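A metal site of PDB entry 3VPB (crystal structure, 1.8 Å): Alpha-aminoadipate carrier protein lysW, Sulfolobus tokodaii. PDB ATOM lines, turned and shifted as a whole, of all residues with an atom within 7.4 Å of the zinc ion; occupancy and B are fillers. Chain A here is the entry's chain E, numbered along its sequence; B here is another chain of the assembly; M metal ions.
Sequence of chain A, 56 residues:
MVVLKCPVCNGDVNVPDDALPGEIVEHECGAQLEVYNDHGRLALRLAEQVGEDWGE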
ATOM      1  N   LYS A   5      29.713   6.570   8.393  1.00  0.00           N
ATOM      2  CA  LYS A   5      29.858   5.538   9.414  1.00  0.00           C
ATOM      3  C   LYS A   5      30.222   6.146  10.766  1.00  0.00           C
ATOM      4  O   LYS A   5      31.083   7.016  10.866  1.00  0.00           O
ATOM      5  CB  LYS A   5      30.875   4.474   9.013  1.00  0.00           C
ATOM      6  CG  LYS A   5      30.374   3.478   7.964  1.00  0.00           C
ATOM      7  CD  LYS A   5      29.272   2.603   8.514  1.00  0.00           C
ATOM      8  CE  LYS A   5      29.301   1.222   7.889  1.00  0.00           C
ATOM      9  NZ  LYS A   5      30.530   0.469   8.340  1.00  0.00           N
ATOM     10  N   CYS A   6      29.542   5.668  11.809  1.00  0.00           N
ATOM     11  CA  CYS A   6      29.843   6.050  13.193  1.00  0.00           C
ATOM     12  C   CYS A   6      31.209   5.503  13.625  1.00  0.00           C
ATOM     13  O   CYS A   6      31.443   4.298  13.555  1.00  0.00           O
ATOM     14  CB  CYS A   6      28.734   5.545  14.104  1.00  0.00           C
ATOM     15  SG  CYS A   6      28.942   5.976  15.838  1.00  0.00           S
ATOM     16  N   PRO A   7      32.114   6.387  14.082  1.00  0.00           N
ATOM     17  CA  PRO A   7      33.460   5.978  14.484  1.00  0.00           C
ATOM     18  C   PRO A   7      33.458   5.187  15.789  1.00  0.00           C
ATOM     19  O   PRO A   7      34.516   4.714  16.247  1.00  0.00           O
ATOM     20  CB  PRO A   7      34.174   7.318  14.679  1.00  0.00           C
ATOM     21  CG  PRO A   7      33.110   8.246  15.107  1.00  0.00           C
ATOM     22  CD  PRO A   7      31.873   7.815  14.355  1.00  0.00           C
ATOM     23  N   VAL A   8      32.279   5.035  16.384  1.00  0.00           N
ATOM     24  CA  VAL A   8      32.118   4.396  17.681  1.00  0.00           C
ATOM     25  C   VAL A   8      31.493   3.014  17.539  1.00  0.00           C
ATOM     26  O   VAL A   8      32.048   2.039  18.050  1.00  0.00           O
ATOM     27  CB  VAL A   8      31.279   5.276  18.648  1.00  0.00           C
ATOM     28  CG1 VAL A   8      30.922   4.516  19.928  1.00  0.00           C
ATOM     29  CG2 VAL A   8      32.025   6.554  18.964  1.00  0.00           C
ATOM     30  N   CYS A   9      30.368   2.932  16.829  1.00  0.00           N
ATOM     31  CA  CYS A   9      29.613   1.682  16.690  1.00  0.00           C
ATOM     32  C   CYS A   9      29.566   1.084  15.280  1.00  0.00           C
ATOM     33  O   CYS A   9      29.087  -0.036  15.094  1.00  0.00           O
ATOM     34  CB  CYS A   9      28.185   1.859  17.195  1.00  0.00           C
ATOM     35  SG  CYS A   9      27.072   2.782  16.102  1.00  0.00           S
ATOM     36  N   ASN A  10      30.038   1.847  14.292  1.00  0.00           N
ATOM     37  CA  ASN A  10      30.027   1.425  12.885  1.00  0.00           C
ATOM     38  C   ASN A  10      28.630   1.302  12.281  1.00  0.00           C
ATOM     39  O   ASN A  10      28.438   0.768  11.186  1.00  0.00           O
ATOM     40  CB  ASN A  10      30.843   0.136  12.687  1.00  0.00           C
ATOM     41  CG  ASN A  10      32.309   0.350  12.957  1.00  0.00           C
ATOM     42  OD1 ASN A  10      33.048  -0.596  13.232  1.00  0.00           O
ATOM     43  ND2 ASN A  10      32.754   1.602  12.867  1.00  0.00           N
ATOM     44  N   GLY A  11      27.640   1.812  13.010  1.00  0.00           N
ATOM     45  CA  GLY A  11      26.291   1.907  12.487  1.00  0.00           C
ATOM     46  C   GLY A  11      26.254   2.939  11.373  1.00  0.00           C
ATOM     47  O   GLY A  11      27.250   3.615  11.097  1.00  0.00           O
ATOM     48  N   ASP A  12      25.105   3.064  10.729  1.00  0.00           N
ATOM     49  CA  ASP A  12      24.955   4.048   9.685  1.00  0.00           C
ATOM     50  C   ASP A  12      24.405   5.330  10.277  1.00  0.00           C
ATOM     51  O   ASP A  12      23.445   5.311  11.054  1.00  0.00           O
ATOM     52  CB  ASP A  12      24.086   3.518   8.530  1.00  0.00           C
ATOM     53  CG  ASP A  12      24.894   2.715   7.499  1.00  0.00           C
ATOM     54  OD1 ASP A  12      26.128   2.595   7.652  1.00  0.00           O
ATOM     55  OD2 ASP A  12      24.289   2.213   6.525  1.00  0.00           O
ATOM     56  N   VAL A  13      25.042   6.454   9.944  1.00  0.00           N
ATOM     57  CA  VAL A  13      24.585   7.757  10.404  1.00  0.00           C
ATOM     58  C   VAL A  13      24.129   8.626   9.229  1.00  0.00           C
ATOM     59  O   VAL A  13      24.905   8.903   8.303  1.00  0.00           O
ATOM     60  CB  VAL A  13      25.651   8.525  11.217  1.00  0.00           C
ATOM     61  CG1 VAL A  13      25.037   9.751  11.897  1.00  0.00           C
ATOM     62  CG2 VAL A  13      26.315   7.626  12.247  1.00  0.00           C
ATOM     63  N   GLU A  26      24.092  13.395  17.216  1.00  0.00           N
ATOM     64  CA  GLU A  26      23.965  12.334  18.196  1.00  0.00           C
ATOM     65  C   GLU A  26      23.641  11.026  17.512  1.00  0.00           C
ATOM     66  O   GLU A  26      22.819  10.996  16.591  1.00  0.00           O
ATOM     67  CB  GLU A  26      22.846  12.654  19.196  1.00  0.00           C
ATOM     68  CG  GLU A  26      23.198  13.759  20.162  1.00  0.00           C
ATOM     69  CD  GLU A  26      23.049  13.335  21.603  1.00  0.00           C
ATOM     70  OE1 GLU A  26      23.396  14.137  22.491  1.00  0.00           O
ATOM     71  OE2 GLU A  26      22.596  12.176  21.838  1.00  0.00           O
ATOM     72  N   HIS A  27      24.296   9.955  17.920  1.00  0.00           N
ATOM     73  CA  HIS A  27      23.979   8.663  17.366  1.00  0.00           C
ATOM     74  C   HIS A  27      23.343   7.757  18.410  1.00  0.00           C
ATOM     75  O   HIS A  27      23.558   7.947  19.613  1.00  0.00           O
ATOM     76  CB  HIS A  27      25.193   8.009  16.715  1.00  0.00           C
ATOM     77  CG  HIS A  27      24.821   6.934  15.740  1.00  0.00           C
ATOM     78  ND1 HIS A  27      25.407   5.691  15.743  1.00  0.00           N
ATOM     79  CD2 HIS A  27      23.877   6.916  14.769  1.00  0.00           C
ATOM     80  CE1 HIS A  27      24.865   4.951  14.783  1.00  0.00           C
ATOM     81  NE2 HIS A  27      23.939   5.670  14.182  1.00  0.00           N
ATOM     82  N   GLU A  28      22.588   6.775  17.927  1.00  0.00           N
ATOM     83  CA  GLU A  28      21.749   5.907  18.770  1.00  0.00           C
ATOM     84  C   GLU A  28      22.557   5.006  19.705  1.00  0.00           C
ATOM     85  O   GLU A  28      22.008   4.433  20.650  1.00  0.00           O
ATOM     86  CB  GLU A  28      20.809   5.067  17.909  1.00  0.00           C
ATOM     87  CG  GLU A  28      21.477   4.528  16.644  1.00  0.00           C
ATOM     88  CD  GLU A  28      20.760   3.355  16.002  1.00  0.00           C
ATOM     89  OE1 GLU A  28      21.478   2.447  15.512  1.00  0.00           O
ATOM     90  OE2 GLU A  28      19.507   3.334  15.976  1.00  0.00           O
ATOM     91  N   CYS A  29      23.849   4.882  19.439  1.00  0.00           N
ATOM     92  CA  CYS A  29      24.769   4.118  20.288  1.00  0.00           C
ATOM     93  C   CYS A  29      25.102   4.825  21.616  1.00  0.00           C
ATOM     94  O   CYS A  29      25.679   4.208  22.521  1.00  0.00           O
ATOM     95  CB  CYS A  29      26.059   3.836  19.532  1.00  0.00           C
ATOM     96  SG  CYS A  29      26.980   5.311  19.052  1.00  0.00           S
ATOM     97  N   GLY A  30      24.794   6.111  21.702  1.00  0.00           N
ATOM     98  CA  GLY A  30      25.121   6.930  22.872  1.00  0.00           C
ATOM     99  C   GLY A  30      26.273   7.909  22.630  1.00  0.00           C
ATOM    100  O   GLY A  30      26.610   8.710  23.513  1.00  0.00           O
ATOM    101  N   ALA A  31      26.880   7.843  21.448  1.00  0.00           N
ATOM    102  CA  ALA A  31      28.005   8.709  21.129  1.00  0.00           C
ATOM    103  C   ALA A  31      27.530  10.068  20.630  1.00  0.00           C
ATOM    104  O   ALA A  31      26.513  10.182  19.935  1.00  0.00           O
ATOM    105  CB  ALA A  31      28.930   8.058  20.107  1.00  0.00           C
ATOM    106  N   LEU A  33      28.941  13.049  18.253  1.00  0.00           N
ATOM    107  CA  LEU A  33      29.865  13.036  17.130  1.00  0.00           C
ATOM    108  C   LEU A  33      29.978  14.423  16.533  1.00  0.00           C
ATOM    109  O   LEU A  33      29.049  15.222  16.635  1.00  0.00           O
ATOM    110  CB  LEU A  33      29.384  12.039  16.045  1.00  0.00           C
ATOM    111  CG  LEU A  33      29.128  10.593  16.518  1.00  0.00           C
ATOM    112  CD1 LEU A  33      28.414   9.734  15.435  1.00  0.00           C
ATOM    113  CD2 LEU A  33      30.413   9.922  16.977  1.00  0.00           C
ATOM    114  N   ILE B   9      27.845   2.623  26.231  1.00  0.00           N
ATOM    115  CA  ILE B   9      27.937   3.040  24.831  1.00  0.00           C
ATOM    116  C   ILE B   9      27.984   1.749  24.009  1.00  0.00           C
ATOM    117  O   ILE B   9      28.841   0.909  24.236  1.00  0.00           O
ATOM    118  CB  ILE B   9      29.224   3.894  24.574  1.00  0.00           C
ATOM    119  CG1 ILE B   9      29.193   5.212  25.384  1.00  0.00           C
ATOM    120  CG2 ILE B   9      29.442   4.144  23.082  1.00  0.00           C
ATOM    121  CD1 ILE B   9      27.913   5.991  25.313  1.00  0.00           C
ATOM    122  N   VAL B  10      27.037   1.581  23.094  1.00  0.00           N
ATOM    123  CA  VAL B  10      26.908   0.308  22.381  1.00  0.00           C
ATOM    124  C   VAL B  10      27.812   0.306  21.147  1.00  0.00           C
ATOM    125  O   VAL B  10      27.441   0.855  20.108  1.00  0.00           O
ATOM    126  CB  VAL B  10      25.430   0.018  22.020  1.00  0.00           C
ATOM    127  CG1 VAL B  10      25.270  -1.225  21.148  1.00  0.00           C
ATOM    128  CG2 VAL B  10      24.596  -0.132  23.281  1.00  0.00           C
ATOM    129  N   ARG B  11      28.982  -0.320  21.263  1.00  0.00           N
ATOM    130  CA  ARG B  11      29.928  -0.458  20.144  1.00  0.00           C
ATOM    131  C   ARG B  11      29.552  -1.690  19.311  1.00  0.00           C
ATOM    132  O   ARG B  11      28.635  -2.431  19.664  1.00  0.00           O
ATOM    133  CB  ARG B  11      31.375  -0.615  20.647  1.00  0.00           C
ATOM    134  CG  ARG B  11      31.962   0.513  21.515  1.00  0.00           C
ATOM    135  CD  ARG B  11      33.213   0.001  22.276  1.00  0.00           C
ATOM    136  NE  ARG B  11      32.907  -1.065  23.249  1.00  0.00           N
ATOM    137  CZ  ARG B  11      33.757  -1.550  24.153  1.00  0.00           C
ATOM    138  NH1 ARG B  11      35.013  -1.103  24.218  1.00  0.00           N
ATOM    139  NH2 ARG B  11      33.349  -2.501  24.996  1.00  0.00           N
ATOM    140  N   LYS B  15      26.742  -4.849  19.989  1.00  0.00           N
ATOM    141  CA  LYS B  15      25.745  -5.184  18.988  1.00  0.00           C
ATOM    142  C   LYS B  15      25.887  -6.643  18.548  1.00  0.00           C
ATOM    143  O   LYS B  15      24.886  -7.321  18.331  1.00  0.00           O
ATOM    144  CB  LYS B  15      25.827  -4.246  17.780  1.00  0.00           C
ATOM    145  CG  LYS B  15      25.490  -2.782  18.094  1.00  0.00           C
ATOM    146  CD  LYS B  15      24.452  -2.228  17.144  1.00  0.00           C
ATOM    147  CE  LYS B  15      25.027  -1.952  15.768  1.00  0.00           C
ATOM    148  NZ  LYS B  15      23.916  -1.826  14.763  1.00  0.00           N
HETATM  149 ZN    ZN M   1      27.160   5.015  16.749  1.00  0.00          ZN
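ND2 of Asn 10 of chain A sits at hydrogen-bond distance from O of Cys 6, at 3.1 Å.
N of Cys 6 lies within hydrogen-bond range of O of Gly 11 of chain A, at 3.2 Å.
The backbone NH (N) of Gly 11 of chain A sits close to the side-chain sulfur (SG) of Cys 9 of chain A (3.3 Å).
O of Asp 12 is in hydrogen-bond range of NE2 of His 27 (3.2 Å).
The side-chain sulfur (SG) of Cys 6 lies close to the backbone NH (N) of Val 8 (3.5 Å).
The side-chain sulfur of Cys 29 sits close to the backbone NH of Ala 31, at 3.5 Å.
N of Val 10 of chain B is in hydrogen-bond range of O of Cys 29, 3.0 Å away.
Of the 20 residues printed, 4 come within 4 Å of the zinc ion.
The zinc ion is bound by ND1 of His 27 (2.1 Å), SG of Cys 6 (2.2 Å), SG of Cys 9 of chain A (2.3 Å) and SG of Cys 29 (2.3 Å).
The zinc ion has four donor atoms within binding distance.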
